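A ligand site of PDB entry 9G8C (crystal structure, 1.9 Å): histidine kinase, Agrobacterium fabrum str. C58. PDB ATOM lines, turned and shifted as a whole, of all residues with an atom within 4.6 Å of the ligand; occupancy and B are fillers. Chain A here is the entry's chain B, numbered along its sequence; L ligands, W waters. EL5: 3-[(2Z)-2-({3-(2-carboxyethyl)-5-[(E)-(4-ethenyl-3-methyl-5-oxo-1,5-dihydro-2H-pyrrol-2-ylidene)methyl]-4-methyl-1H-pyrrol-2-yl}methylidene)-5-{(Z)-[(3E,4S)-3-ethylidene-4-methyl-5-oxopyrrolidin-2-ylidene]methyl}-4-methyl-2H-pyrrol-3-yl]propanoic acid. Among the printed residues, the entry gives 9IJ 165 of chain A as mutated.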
ATOM      1  N   LEU A  10       7.248  28.731 -14.484  1.00  0.00           N
ATOM      2  CA  LEU A  10       6.377  28.006 -13.527  1.00  0.00           C
ATOM      3  C   LEU A  10       6.264  28.799 -12.207  1.00  0.00           C
ATOM      4  O   LEU A  10       5.297  28.530 -11.466  1.00  0.00           O
ATOM      5  CB  LEU A  10       6.919  26.602 -13.277  1.00  0.00           C
ATOM      6  CG  LEU A  10       6.936  25.672 -14.493  1.00  0.00           C
ATOM      7  CD1 LEU A  10       7.321  24.259 -14.089  1.00  0.00           C
ATOM      8  CD2 LEU A  10       5.595  25.674 -15.208  1.00  0.00           C
ATOM      9  N   CYS A  13       3.654  32.017 -13.727  1.00  0.00           N
ATOM     10  CA  CYS A  13       2.548  31.774 -14.705  1.00  0.00           C
ATOM     11  C   CYS A  13       1.174  31.950 -14.038  1.00  0.00           C
ATOM     12  O   CYS A  13       0.204  32.284 -14.765  1.00  0.00           O
ATOM     13  CB  CYS A  13       2.688  30.414 -15.394  1.00  0.00           C
ATOM     14  SG  CYS A  13       2.613  28.987 -14.294  1.00  0.00           S
ATOM     15  N   ASP A  14       1.083  31.844 -12.711  1.00  0.00           N
ATOM     16  CA  ASP A  14      -0.177  32.089 -11.939  1.00  0.00           C
ATOM     17  C   ASP A  14      -0.649  33.548 -12.110  1.00  0.00           C
ATOM     18  O   ASP A  14      -1.847  33.799 -11.827  1.00  0.00           O
ATOM     19  CB  ASP A  14      -0.012  31.703 -10.467  1.00  0.00           C
ATOM     20  CG  ASP A  14       0.969  32.536  -9.664  1.00  0.00           C
ATOM     21  OD1 ASP A  14       1.696  33.340 -10.273  1.00  0.00           O
ATOM     22  OD2 ASP A  14       1.004  32.373  -8.427  1.00  0.00           O
ATOM     23  N   ILE A  18      -2.116  37.525 -19.597  1.00  0.00           N
ATOM     24  CA  ILE A  18      -2.447  36.794 -20.868  1.00  0.00           C
ATOM     25  C   ILE A  18      -3.451  37.599 -21.702  1.00  0.00           C
ATOM     26  O   ILE A  18      -3.710  37.199 -22.850  1.00  0.00           O
ATOM     27  CB  ILE A  18      -2.925  35.364 -20.555  1.00  0.00           C
ATOM     28  CG1 ILE A  18      -4.132  35.340 -19.615  1.00  0.00           C
ATOM     29  CG2 ILE A  18      -1.771  34.536 -20.011  1.00  0.00           C
ATOM     30  CD1 ILE A  18      -4.878  34.024 -19.561  1.00  0.00           C
ATOM     31  N   9IJ A 165     -15.293  18.990 -19.230  1.00  0.00           N
ATOM     32  CA  9IJ A 165     -14.879  18.866 -17.833  1.00  0.00           C
ATOM     33  C   9IJ A 165     -15.754  19.718 -16.894  1.00  0.00           C
ATOM     34  CB  9IJ A 165     -13.403  19.109 -17.639  1.00  0.00           C
ATOM     35  CG  9IJ A 165     -12.897  20.515 -17.896  1.00  0.00           C
ATOM     36  CD1 9IJ A 165     -13.103  21.508 -16.943  1.00  0.00           C
ATOM     37  CD2 9IJ A 165     -12.172  20.786 -19.045  1.00  0.00           C
ATOM     38  CE1 9IJ A 165     -12.607  22.810 -17.169  1.00  0.00           C
ATOM     39  CE2 9IJ A 165     -11.697  22.093 -19.270  1.00  0.00           C
ATOM     40  CZ  9IJ A 165     -11.902  23.089 -18.326  1.00  0.00           C
ATOM     41  C01 9IJ A 165     -11.956  19.870 -19.943  1.00  0.00           C
ATOM     42  N01 9IJ A 165     -11.751  18.993 -20.682  1.00  0.00           N
ATOM     43  O   9IJ A 165     -16.267  20.897 -17.486  1.00  0.00           O
ATOM     44  N   PHE A 187      -8.724  10.283 -21.244  1.00  0.00           N
ATOM     45  CA  PHE A 187      -8.665  11.144 -20.038  1.00  0.00           C
ATOM     46  C   PHE A 187      -9.977  11.067 -19.260  1.00  0.00           C
ATOM     47  O   PHE A 187     -10.150  11.833 -18.293  1.00  0.00           O
ATOM     48  CB  PHE A 187      -8.362  12.597 -20.427  1.00  0.00           C
ATOM     49  CG  PHE A 187      -7.057  12.814 -21.162  1.00  0.00           C
ATOM     50  CD1 PHE A 187      -5.860  12.364 -20.627  1.00  0.00           C
ATOM     51  CD2 PHE A 187      -7.021  13.507 -22.361  1.00  0.00           C
ATOM     52  CE1 PHE A 187      -4.660  12.594 -21.285  1.00  0.00           C
ATOM     53  CE2 PHE A 187      -5.823  13.727 -23.022  1.00  0.00           C
ATOM     54  CZ  PHE A 187      -4.640  13.258 -22.483  1.00  0.00           C
ATOM     55  N   GLN A 190     -10.407  11.439 -15.235  1.00  0.00           N
ATOM     56  CA  GLN A 190      -9.174  12.124 -14.780  1.00  0.00           C
ATOM     57  C   GLN A 190      -9.546  13.478 -14.167  1.00  0.00           C
ATOM     58  O   GLN A 190     -10.569  14.065 -14.555  1.00  0.00           O
ATOM     59  CB  GLN A 190      -8.246  12.309 -15.986  1.00  0.00           C
ATOM     60  CG  GLN A 190      -6.847  12.753 -15.615  1.00  0.00           C
ATOM     61  CD  GLN A 190      -5.819  12.326 -16.622  1.00  0.00           C
ATOM     62  OE1 GLN A 190      -5.896  11.248 -17.214  1.00  0.00           O
ATOM     63  NE2 GLN A 190      -4.807  13.167 -16.779  1.00  0.00           N
ATOM     64  N   PHE A 192      -7.593  17.403 -12.977  1.00  0.00           N
ATOM     65  CA  PHE A 192      -6.411  18.303 -12.937  1.00  0.00           C
ATOM     66  C   PHE A 192      -6.620  19.325 -11.829  1.00  0.00           C
ATOM     67  O   PHE A 192      -7.753  19.731 -11.541  1.00  0.00           O
ATOM     68  CB  PHE A 192      -6.155  18.969 -14.291  1.00  0.00           C
ATOM     69  CG  PHE A 192      -7.341  19.675 -14.904  1.00  0.00           C
ATOM     70  CD1 PHE A 192      -7.650  20.972 -14.538  1.00  0.00           C
ATOM     71  CD2 PHE A 192      -8.132  19.045 -15.853  1.00  0.00           C
ATOM     72  CE1 PHE A 192      -8.729  21.640 -15.111  1.00  0.00           C
ATOM     73  CE2 PHE A 192      -9.211  19.709 -16.416  1.00  0.00           C
ATOM     74  CZ  PHE A 192      -9.498  21.011 -16.049  1.00  0.00           C
ATOM     75  N   SER A 195      -4.773  24.912 -10.296  1.00  0.00           N
ATOM     76  CA  SER A 195      -3.635  25.762 -10.754  1.00  0.00           C
ATOM     77  C   SER A 195      -3.314  25.529 -12.247  1.00  0.00           C
ATOM     78  O   SER A 195      -2.561  26.350 -12.829  1.00  0.00           O
ATOM     79  CB  SER A 195      -2.435  25.549  -9.905  1.00  0.00           C
ATOM     80  OG  SER A 195      -2.003  24.214 -10.000  1.00  0.00           O
ATOM     81  N   ASP A 196      -3.872  24.468 -12.857  1.00  0.00           N
ATOM     82  CA  ASP A 196      -3.686  24.167 -14.298  1.00  0.00           C
ATOM     83  C   ASP A 196      -4.382  25.240 -15.132  1.00  0.00           C
ATOM     84  O   ASP A 196      -4.002  25.400 -16.306  1.00  0.00           O
ATOM     85  CB  ASP A 196      -4.210  22.778 -14.674  1.00  0.00           C
ATOM     86  CG  ASP A 196      -3.167  21.686 -14.441  1.00  0.00           C
ATOM     87  OD1 ASP A 196      -2.217  21.941 -13.690  1.00  0.00           O
ATOM     88  OD2 ASP A 196      -3.327  20.604 -15.025  1.00  0.00           O
ATOM     89  N   ILE A 197      -5.381  25.923 -14.559  1.00  0.00           N
ATOM     90  CA  ILE A 197      -6.072  27.059 -15.217  1.00  0.00           C
ATOM     91  C   ILE A 197      -5.984  28.265 -14.282  1.00  0.00           C
ATOM     92  O   ILE A 197      -6.758  28.380 -13.339  1.00  0.00           O
ATOM     93  CB  ILE A 197      -7.521  26.725 -15.627  1.00  0.00           C
ATOM     94  CG1 ILE A 197      -7.638  25.371 -16.337  1.00  0.00           C
ATOM     95  CG2 ILE A 197      -8.050  27.864 -16.493  1.00  0.00           C
ATOM     96  CD1 ILE A 197      -9.025  25.014 -16.827  1.00  0.00           C
ATOM     97  N   PRO A 198      -5.067  29.221 -14.561  1.00  0.00           N
ATOM     98  CA  PRO A 198      -4.881  30.380 -13.692  1.00  0.00           C
ATOM     99  C   PRO A 198      -6.112  31.301 -13.706  1.00  0.00           C
ATOM    100  O   PRO A 198      -6.941  31.170 -14.606  1.00  0.00           O
ATOM    101  CB  PRO A 198      -3.632  31.105 -14.218  1.00  0.00           C
ATOM    102  CG  PRO A 198      -3.329  30.479 -15.571  1.00  0.00           C
ATOM    103  CD  PRO A 198      -4.147  29.216 -15.700  1.00  0.00           C
ATOM    104  N   ALA A 201      -7.107  33.282 -16.867  1.00  0.00           N
ATOM    105  CA  ALA A 201      -7.666  32.389 -17.917  1.00  0.00           C
ATOM    106  C   ALA A 201      -9.147  32.108 -17.600  1.00  0.00           C
ATOM    107  O   ALA A 201      -9.988  32.199 -18.516  1.00  0.00           O
ATOM    108  CB  ALA A 201      -6.837  31.133 -18.028  1.00  0.00           C
ATOM    109  N   TYR A 205     -12.349  32.871 -19.854  1.00  0.00           N
ATOM    110  CA  TYR A 205     -13.316  31.801 -20.249  1.00  0.00           C
ATOM    111  C   TYR A 205     -14.726  32.268 -19.869  1.00  0.00           C
ATOM    112  O   TYR A 205     -15.680  31.892 -20.573  1.00  0.00           O
ATOM    113  CB  TYR A 205     -12.957  30.440 -19.640  1.00  0.00           C
ATOM    114  CG  TYR A 205     -11.754  29.759 -20.243  1.00  0.00           C
ATOM    115  CD1 TYR A 205     -11.673  29.468 -21.598  1.00  0.00           C
ATOM    116  CD2 TYR A 205     -10.694  29.346 -19.436  1.00  0.00           C
ATOM    117  CE1 TYR A 205     -10.568  28.834 -22.134  1.00  0.00           C
ATOM    118  CE2 TYR A 205      -9.577  28.716 -19.960  1.00  0.00           C
ATOM    119  CZ  TYR A 205      -9.513  28.442 -21.320  1.00  0.00           C
ATOM    120  OH  TYR A 205      -8.413  27.825 -21.841  1.00  0.00           O
ATOM    121  N   ARG A 211     -12.947  30.077 -27.095  1.00  0.00           N
ATOM    122  CA  ARG A 211     -11.485  30.325 -27.119  1.00  0.00           C
ATOM    123  C   ARG A 211     -10.875  29.432 -28.197  1.00  0.00           C
ATOM    124  O   ARG A 211     -11.002  28.199 -28.073  1.00  0.00           O
ATOM    125  CB  ARG A 211     -10.876  30.073 -25.740  1.00  0.00           C
ATOM    126  CG  ARG A 211      -9.359  30.185 -25.712  1.00  0.00           C
ATOM    127  CD  ARG A 211      -8.849  31.479 -26.307  1.00  0.00           C
ATOM    128  NE  ARG A 211      -7.437  31.681 -26.000  1.00  0.00           N
ATOM    129  CZ  ARG A 211      -6.628  32.567 -26.593  1.00  0.00           C
ATOM    130  NH1 ARG A 211      -7.067  33.325 -27.586  1.00  0.00           N
ATOM    131  NH2 ARG A 211      -5.378  32.663 -26.194  1.00  0.00           N
ATOM    132  N   ILE A 213      -7.498  28.275 -30.497  1.00  0.00           N
ATOM    133  CA  ILE A 213      -6.027  28.126 -30.737  1.00  0.00           C
ATOM    134  C   ILE A 213      -5.869  27.403 -32.078  1.00  0.00           C
ATOM    135  O   ILE A 213      -6.242  26.224 -32.138  1.00  0.00           O
ATOM    136  CB  ILE A 213      -5.349  27.375 -29.574  1.00  0.00           C
ATOM    137  CG1 ILE A 213      -5.636  28.027 -28.214  1.00  0.00           C
ATOM    138  CG2 ILE A 213      -3.842  27.248 -29.807  1.00  0.00           C
ATOM    139  CD1 ILE A 213      -4.983  27.305 -27.053  1.00  0.00           C
ATOM    140  N   ARG A 242      -6.327  36.745 -30.247  1.00  0.00           N
ATOM    141  CA  ARG A 242      -5.339  36.925 -29.143  1.00  0.00           C
ATOM    142  C   ARG A 242      -4.416  35.704 -29.023  1.00  0.00           C
ATOM    143  O   ARG A 242      -4.943  34.549 -29.003  1.00  0.00           O
ATOM    144  CB  ARG A 242      -6.065  37.191 -27.818  1.00  0.00           C
ATOM    145  CG  ARG A 242      -5.132  37.237 -26.619  1.00  0.00           C
ATOM    146  CD  ARG A 242      -5.862  37.641 -25.357  1.00  0.00           C
ATOM    147  NE  ARG A 242      -6.983  36.746 -25.113  1.00  0.00           N
ATOM    148  CZ  ARG A 242      -6.919  35.633 -24.377  1.00  0.00           C
ATOM    149  NH1 ARG A 242      -5.803  35.296 -23.755  1.00  0.00           N
ATOM    150  NH2 ARG A 242      -8.004  34.885 -24.254  1.00  0.00           N
ATOM    151  N   VAL A 244      -1.444  32.947 -27.475  1.00  0.00           N
ATOM    152  CA  VAL A 244      -1.575  31.954 -26.378  1.00  0.00           C
ATOM    153  C   VAL A 244      -0.327  31.991 -25.506  1.00  0.00           C
ATOM    154  O   VAL A 244       0.766  32.130 -26.066  1.00  0.00           O
ATOM    155  CB  VAL A 244      -1.799  30.532 -26.920  1.00  0.00           C
ATOM    156  CG1 VAL A 244      -2.088  29.556 -25.788  1.00  0.00           C
ATOM    157  CG2 VAL A 244      -2.878  30.480 -27.986  1.00  0.00           C
ATOM    158  N   SER A 245      -0.517  31.857 -24.187  1.00  0.00           N
ATOM    159  CA  SER A 245       0.587  31.680 -23.203  1.00  0.00           C
ATOM    160  C   SER A 245       1.567  30.609 -23.685  1.00  0.00           C
ATOM    161  O   SER A 245       1.141  29.504 -24.015  1.00  0.00           O
ATOM    162  CB  SER A 245       0.061  31.315 -21.841  1.00  0.00           C
ATOM    163  OG  SER A 245       1.121  30.854 -21.017  1.00  0.00           O
ATOM    164  N   ILE A 247       3.336  28.830 -21.767  1.00  0.00           N
ATOM    165  CA  ILE A 247       3.141  27.728 -20.788  1.00  0.00           C
ATOM    166  C   ILE A 247       2.126  26.724 -21.361  1.00  0.00           C
ATOM    167  O   ILE A 247       2.442  25.516 -21.459  1.00  0.00           O
ATOM    168  CB  ILE A 247       2.662  28.254 -19.425  1.00  0.00           C
ATOM    169  CG1 ILE A 247       3.630  29.263 -18.799  1.00  0.00           C
ATOM    170  CG2 ILE A 247       2.381  27.098 -18.484  1.00  0.00           C
ATOM    171  CD1 ILE A 247       5.033  28.722 -18.584  1.00  0.00           C
ATOM    172  N   HIS A 248       0.949  27.222 -21.756  1.00  0.00           N
ATOM    173  CA  HIS A 248      -0.116  26.363 -22.337  1.00  0.00           C
ATOM    174  C   HIS A 248       0.330  25.776 -23.687  1.00  0.00           C
ATOM    175  O   HIS A 248       0.045  24.587 -23.927  1.00  0.00           O
ATOM    176  CB  HIS A 248      -1.434  27.123 -22.495  1.00  0.00           C
ATOM    177  CG  HIS A 248      -2.558  26.207 -22.842  1.00  0.00           C
ATOM    178  ND1 HIS A 248      -2.865  25.120 -22.068  1.00  0.00           N
ATOM    179  CD2 HIS A 248      -3.419  26.201 -23.882  1.00  0.00           C
ATOM    180  CE1 HIS A 248      -3.890  24.476 -22.614  1.00  0.00           C
ATOM    181  NE2 HIS A 248      -4.247  25.131 -23.722  1.00  0.00           N
ATOM    182  N   TYR A 251       2.418  22.918 -22.884  1.00  0.00           N
ATOM    183  CA  TYR A 251       1.552  21.839 -22.350  1.00  0.00           C
ATOM    184  C   TYR A 251       0.931  21.078 -23.538  1.00  0.00           C
ATOM    185  O   TYR A 251       1.015  19.829 -23.597  1.00  0.00           O
ATOM    186  CB  TYR A 251       0.476  22.395 -21.409  1.00  0.00           C
ATOM    187  CG  TYR A 251      -0.093  21.375 -20.468  1.00  0.00           C
ATOM    188  CD1 TYR A 251      -0.838  20.311 -20.954  1.00  0.00           C
ATOM    189  CD2 TYR A 251       0.128  21.446 -19.096  1.00  0.00           C
ATOM    190  CE1 TYR A 251      -1.341  19.335 -20.105  1.00  0.00           C
ATOM    191  CE2 TYR A 251      -0.374  20.477 -18.234  1.00  0.00           C
ATOM    192  CZ  TYR A 251      -1.099  19.414 -18.741  1.00  0.00           C
ATOM    193  OH  TYR A 251      -1.607  18.429 -17.926  1.00  0.00           O
ATOM    194  N   MET A 255       1.434  17.096 -25.009  1.00  0.00           N
ATOM    195  CA  MET A 255       0.287  16.179 -25.232  1.00  0.00           C
ATOM    196  C   MET A 255       0.310  15.665 -26.687  1.00  0.00           C
ATOM    197  O   MET A 255      -0.245  14.592 -26.913  1.00  0.00           O
ATOM    198  CB  MET A 255      -1.048  16.882 -24.978  1.00  0.00           C
ATOM    199  CG  MET A 255      -1.294  17.178 -23.507  1.00  0.00           C
ATOM    200  SD  MET A 255      -2.809  18.149 -23.319  1.00  0.00           S
ATOM    201  CE  MET A 255      -4.031  16.865 -23.581  1.00  0.00           C
ATOM    202  N   SER A 260      -7.009  23.849 -30.652  1.00  0.00           N
ATOM    203  CA  SER A 260      -8.146  23.640 -29.726  1.00  0.00           C
ATOM    204  C   SER A 260      -9.219  24.692 -29.981  1.00  0.00           C
ATOM    205  O   SER A 260      -8.924  25.731 -30.624  1.00  0.00           O
ATOM    206  CB  SER A 260      -7.699  23.601 -28.282  1.00  0.00           C
ATOM    207  OG  SER A 260      -7.289  24.870 -27.808  1.00  0.00           O
ATOM    208  N   LEU A 274     -15.954  23.521 -19.242  1.00  0.00           N
ATOM    209  CA  LEU A 274     -15.743  23.745 -20.700  1.00  0.00           C
ATOM    210  C   LEU A 274     -16.137  22.500 -21.471  1.00  0.00           C
ATOM    211  O   LEU A 274     -15.955  21.385 -20.965  1.00  0.00           O
ATOM    212  CB  LEU A 274     -14.265  24.050 -20.989  1.00  0.00           C
ATOM    213  CG  LEU A 274     -13.673  25.297 -20.343  1.00  0.00           C
ATOM    214  CD1 LEU A 274     -12.224  25.440 -20.817  1.00  0.00           C
ATOM    215  CD2 LEU A 274     -14.462  26.548 -20.704  1.00  0.00           C
ATOM    216  N   ALA A 276     -14.234  21.220 -24.357  1.00  0.00           N
ATOM    217  CA  ALA A 276     -12.867  21.386 -24.909  1.00  0.00           C
ATOM    218  C   ALA A 276     -12.717  20.503 -26.142  1.00  0.00           C
ATOM    219  O   ALA A 276     -12.792  19.224 -26.012  1.00  0.00           O
ATOM    220  CB  ALA A 276     -11.846  21.048 -23.859  1.00  0.00           C
ATOM    221  N   HIS A 278     -10.017  19.320 -28.965  1.00  0.00           N
ATOM    222  CA  HIS A 278      -8.550  19.238 -29.174  1.00  0.00           C
ATOM    223  C   HIS A 278      -8.268  18.564 -30.531  1.00  0.00           C
ATOM    224  O   HIS A 278      -8.960  17.591 -30.832  1.00  0.00           O
ATOM    225  CB  HIS A 278      -7.855  18.482 -28.044  1.00  0.00           C
ATOM    226  CG  HIS A 278      -7.819  19.212 -26.743  1.00  0.00           C
ATOM    227  ND1 HIS A 278      -7.299  18.635 -25.600  1.00  0.00           N
ATOM    228  CD2 HIS A 278      -8.234  20.454 -26.394  1.00  0.00           C
ATOM    229  CE1 HIS A 278      -7.384  19.510 -24.600  1.00  0.00           C
ATOM    230  NE2 HIS A 278      -7.962  20.633 -25.062  1.00  0.00           N
ATOM    231  N   ARG A 456       6.124  19.097 -15.322  1.00  0.00           N
ATOM    232  CA  ARG A 456       4.942  19.791 -14.746  1.00  0.00           C
ATOM    233  C   ARG A 456       3.845  19.887 -15.818  1.00  0.00           C
ATOM    234  O   ARG A 456       2.661  19.686 -15.476  1.00  0.00           O
ATOM    235  CB  ARG A 456       5.303  21.180 -14.203  1.00  0.00           C
ATOM    236  CG  ARG A 456       4.101  22.005 -13.755  1.00  0.00           C
ATOM    237  CD  ARG A 456       3.334  21.367 -12.604  1.00  0.00           C
ATOM    238  NE  ARG A 456       2.175  22.158 -12.187  1.00  0.00           N
ATOM    239  CZ  ARG A 456       0.952  22.088 -12.725  1.00  0.00           C
ATOM    240  NH1 ARG A 456       0.697  21.251 -13.715  1.00  0.00           N
ATOM    241  NH2 ARG A 456      -0.012  22.870 -12.258  1.00  0.00           N
ATOM    242  N   LEU A 457       4.214  20.157 -17.063  1.00  0.00           N
ATOM    243  CA  LEU A 457       3.230  20.483 -18.137  1.00  0.00           C
ATOM    244  C   LEU A 457       2.831  19.213 -18.895  1.00  0.00           C
ATOM    245  O   LEU A 457       2.893  19.215 -20.139  1.00  0.00           O
ATOM    246  CB  LEU A 457       3.840  21.540 -19.056  1.00  0.00           C
ATOM    247  CG  LEU A 457       4.273  22.846 -18.371  1.00  0.00           C
ATOM    248  CD1 LEU A 457       4.826  23.818 -19.389  1.00  0.00           C
ATOM    249  CD2 LEU A 457       3.122  23.487 -17.613  1.00  0.00           C
ATOM    250  N   PRO A 459      -0.270  15.748 -18.671  1.00  0.00           N
ATOM    251  CA  PRO A 459      -1.441  15.183 -17.990  1.00  0.00           C
ATOM    252  C   PRO A 459      -1.115  14.202 -16.847  1.00  0.00           C
ATOM    253  O   PRO A 459      -1.810  14.198 -15.857  1.00  0.00           O
ATOM    254  CB  PRO A 459      -2.206  14.498 -19.134  1.00  0.00           C
ATOM    255  CG  PRO A 459      -1.832  15.329 -20.353  1.00  0.00           C
ATOM    256  CD  PRO A 459      -0.365  15.620 -20.133  1.00  0.00           C
ATOM    257  N   SER A 462      -0.048  16.437 -13.961  1.00  0.00           N
ATOM    258  CA  SER A 462      -1.227  17.185 -13.526  1.00  0.00           C
ATOM    259  C   SER A 462      -2.062  16.269 -12.606  1.00  0.00           C
ATOM    260  O   SER A 462      -2.467  16.702 -11.523  1.00  0.00           O
ATOM    261  CB  SER A 462      -2.060  17.705 -14.687  1.00  0.00           C
ATOM    262  OG  SER A 462      -1.446  18.825 -15.293  1.00  0.00           O
HETATM  263  C1A EL5 L   1      -0.508  24.887 -16.389  1.00  0.00           C
HETATM  264  C1B EL5 L   1      -2.821  27.911 -18.669  1.00  0.00           C
HETATM  265  O1B EL5 L   1      -6.353  29.575 -24.320  1.00  0.00           O
HETATM  266  C1C EL5 L   1      -5.790  25.000 -19.896  1.00  0.00           C
HETATM  267  O1C EL5 L   1      -9.405  22.531 -22.005  1.00  0.00           O
HETATM  268  C1D EL5 L   1      -5.013  20.431 -18.629  1.00  0.00           C
HETATM  269  C2A EL5 L   1       0.091  25.848 -15.590  1.00  0.00           C
HETATM  270  C2B EL5 L   1      -3.309  28.972 -19.422  1.00  0.00           C
HETATM  271  O2B EL5 L   1      -5.041  31.213 -23.604  1.00  0.00           O
HETATM  272  C2C EL5 L   1      -6.948  24.243 -20.070  1.00  0.00           C
HETATM  273  O2C EL5 L   1      -8.399  23.043 -23.916  1.00  0.00           O
HETATM  274  C2D EL5 L   1      -5.411  19.621 -19.695  1.00  0.00           C
HETATM  275  C3A EL5 L   1      -0.227  27.145 -15.988  1.00  0.00           C
HETATM  276  C3B EL5 L   1      -4.397  28.506 -20.144  1.00  0.00           C
HETATM  277  C3C EL5 L   1      -6.724  23.015 -19.473  1.00  0.00           C
HETATM  278  C3D EL5 L   1      -5.269  18.305 -19.272  1.00  0.00           C
HETATM  279  C4A EL5 L   1      -1.149  26.959 -17.021  1.00  0.00           C
HETATM  280  C4B EL5 L   1      -4.597  27.186 -19.745  1.00  0.00           C
HETATM  281  C4C EL5 L   1      -5.399  22.938 -19.064  1.00  0.00           C
HETATM  282  C4D EL5 L   1      -4.754  18.298 -17.986  1.00  0.00           C
HETATM  283  CAA EL5 L   1       0.210  28.357 -15.385  1.00  0.00           C
HETATM  284  CAB EL5 L   1      -5.209  29.253 -21.152  1.00  0.00           C
HETATM  285  CAC EL5 L   1      -8.243  24.695 -20.678  1.00  0.00           C
HETATM  286  CAD EL5 L   1      -5.565  17.174 -20.039  1.00  0.00           C
HETATM  287  CBA EL5 L   1       0.994  28.501 -14.281  1.00  0.00           C
HETATM  288  CBB EL5 L   1      -4.787  29.048 -22.605  1.00  0.00           C
HETATM  289  CBC EL5 L   1      -8.360  24.664 -22.194  1.00  0.00           C
HETATM  290  CBD EL5 L   1      -5.465  15.921 -19.680  1.00  0.00           C
HETATM  291  CGB EL5 L   1      -5.434  30.015 -23.586  1.00  0.00           C
HETATM  292  CGC EL5 L   1      -8.745  23.306 -22.748  1.00  0.00           C
HETATM  293  CHB EL5 L   1      -1.819  27.970 -17.707  1.00  0.00           C
HETATM  294  CHC EL5 L   1      -5.538  26.316 -20.287  1.00  0.00           C
HETATM  295  CHD EL5 L   1      -4.965  21.805 -18.417  1.00  0.00           C
HETATM  296  CMA EL5 L   1       1.354  25.530 -14.837  1.00  0.00           C
HETATM  297  CMB EL5 L   1      -2.743  30.361 -19.497  1.00  0.00           C
HETATM  298  CMC EL5 L   1      -7.737  21.918 -19.395  1.00  0.00           C
HETATM  299  CMD EL5 L   1      -5.884  20.057 -21.048  1.00  0.00           C
HETATM  300  NA  EL5 L   1      -1.289  25.601 -17.281  1.00  0.00           N
HETATM  301  OA  EL5 L   1      -0.374  23.694 -16.358  1.00  0.00           O
HETATM  302  NB  EL5 L   1      -3.651  26.831 -18.826  1.00  0.00           N
HETATM  303  NC  EL5 L   1      -4.895  24.215 -19.214  1.00  0.00           N
HETATM  304  ND  EL5 L   1      -4.580  19.594 -17.619  1.00  0.00           N
HETATM  305  OD  EL5 L   1      -4.473  17.364 -17.236  1.00  0.00           O
HETATM  306  O   HOH W   1      -1.984  24.055 -19.558  1.00  0.00           O
HETATM  307  O   HOH W   2      -4.909  15.517 -15.179  1.00  0.00           O
HETATM  308  O   HOH W   3      -7.807  27.325 -24.472  1.00  0.00           O
HETATM  309  O   HOH W   4     -10.186  23.664 -25.865  1.00  0.00           O
HETATM  310  O   HOH W   5      -0.699  31.774 -17.205  1.00  0.00           O
HETATM  311  O   HOH W   6      -2.891  32.466 -22.867  1.00  0.00           O
HETATM  312  O   HOH W   7      -6.947  32.982 -22.586  1.00  0.00           O
HETATM  313  O   HOH W   8      -6.699  24.684 -25.091  1.00  0.00           O
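Asp 14 touches the ligand.
CE2 of 9IJ 165 touches O1C of the ligand, 3.6 Å away.
Phe 187 touches the ligand.
Phe 192 touches the ligand.
Ser 195 touches the ligand (O to C2A, 3.9 Å).
Ile 197 touches the ligand.
Pro 198 touches the ligand.
CB of Ala 201 touches CAB of the ligand, 3.99 Å away.
Tyr 205 touches the ligand (OH to CBC, 3.2 Å).
Ile 213 touches the ligand (CD1 to O1B, 3.8 Å).
Ser 245 touches the ligand (CB to CMB, 3.8 Å).
Ile 247 touches the ligand (CG2 to C3A, 3.6 Å).
His 248 touches the ligand.
CE of Met 255 touches CAD of the ligand, 3.9 Å away.
CB of Ala 276 touches O1C of the ligand (3.4 Å).
NH1 of Arg 456 touches OA of the ligand (3.8 Å).
Leu 457 touches the ligand (CD2 to OA, 3.7 Å).
Pro 459 touches the ligand (CB to CBD, 3.6 Å).
Ser 462 touches the ligand.
Hydrophobic or aromatic side chains that line the ligand: Phe 187, Phe 192, Ile 197, Pro 198, Ala 201, Ile 213, Ile 247, His 248, Tyr 251, Met 255, Ala 276, His 278, Leu 457 and Pro 459.
24 residues have an atom within 4 Å of the ligand: Cys 13, Asp 14, 9IJ 165, Phe 187, Phe 192, Ser 195, Asp 196, Ile 197, Pro 198, Ala 201, Tyr 205, Arg 211, Ile 213, Ser 245, Ile 247, His 248, Tyr 251, Met 255, Ala 276, His 278, Arg 456, Leu 457, Pro 459 and Ser 462.
The nearest printed residue that does not touch the ligand is Val 244 (4.03 Å).
A ring nitrogen (NE2) of His 278 is in hydrogen-bond range of an oxygen (O2C) of the ligand.
The guanidinium group (NE) of Arg 211 is in salt-bridge range of an oxygen (O1B) of the ligand.
The side-chain hydroxyl of Tyr 251 lies within hydrogen-bond range of an oxygen (OD) of the ligand (3.1 Å).
SG of Cys 13 is bonded to CBA of the ligand (1.7 Å).
The backbone carbonyl oxygen (O) of Asp 196 is in hydrogen-bond range of a nitrogen (NA) of the ligand (2.9 Å).
A nitrogen (ND) of the ligand sits at hydrogen-bond distance from the side-chain carboxylate (OD2) of Asp 196, 3.1 Å away.
Water W6 lies within hydrogen-bond range of an oxygen (O2B) of the ligand (2.6 Å) and the backbone NH (N) of Ser 245 (2.8 Å).
Water W8 lies within hydrogen-bond range of an oxygen (O2C) of the ligand (2.6 Å), the side-chain hydroxyl (OG) of Ser 260 (2.8 Å) and a ring nitrogen (NE2) of His 248 (2.8 Å).
Water W3 lies within hydrogen-bond range of O1B of the ligand and OH of Tyr 205.
Water W7 lies within hydrogen-bond range of the guanidinium group (NH2) of Arg 242 (2.7 Å) and an oxygen (O2B) of the ligand (2.8 Å).
Water W2 lies within hydrogen-bond range of an oxygen (OD) of the ligand (2.8 Å), the side-chain amide nitrogen (NE2) of Gln 190 (2.8 Å) and the backbone carbonyl oxygen (O) of Pro 459 (3.4 Å).
Water W1 bridges a nitrogen (NA) of the ligand (2.8 Å) and a ring nitrogen (ND1) of His 248 (2.9 Å).
O of Arg 242 sits at hydrogen-bond distance from NH1 of Arg 211 (2.8 Å).
OG of Ser 195 sits at hydrogen-bond distance from NH2 of Arg 456 (3.3 Å).
The side-chain hydroxyl (OG) of Ser 462 sits at hydrogen-bond distance from the side-chain carboxylate (OD2) of Asp 196 (2.6 Å).
O of Pro 459 sits at hydrogen-bond distance from NE2 of Gln 190 (3.3 Å).
N of Ile 247 is in hydrogen-bond range of OG of Ser 245 (3.1 Å).
The side-chain hydroxyl (OG) of Ser 462 is in hydrogen-bond range of the side-chain hydroxyl (OH) of Tyr 251, 2.7 Å away.
The backbone carbonyl oxygen of Ile 213 sits at hydrogen-bond distance from the backbone NH of Ser 260.
N of 9IJ 165 lies within hydrogen-bond range of O of Leu 274.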
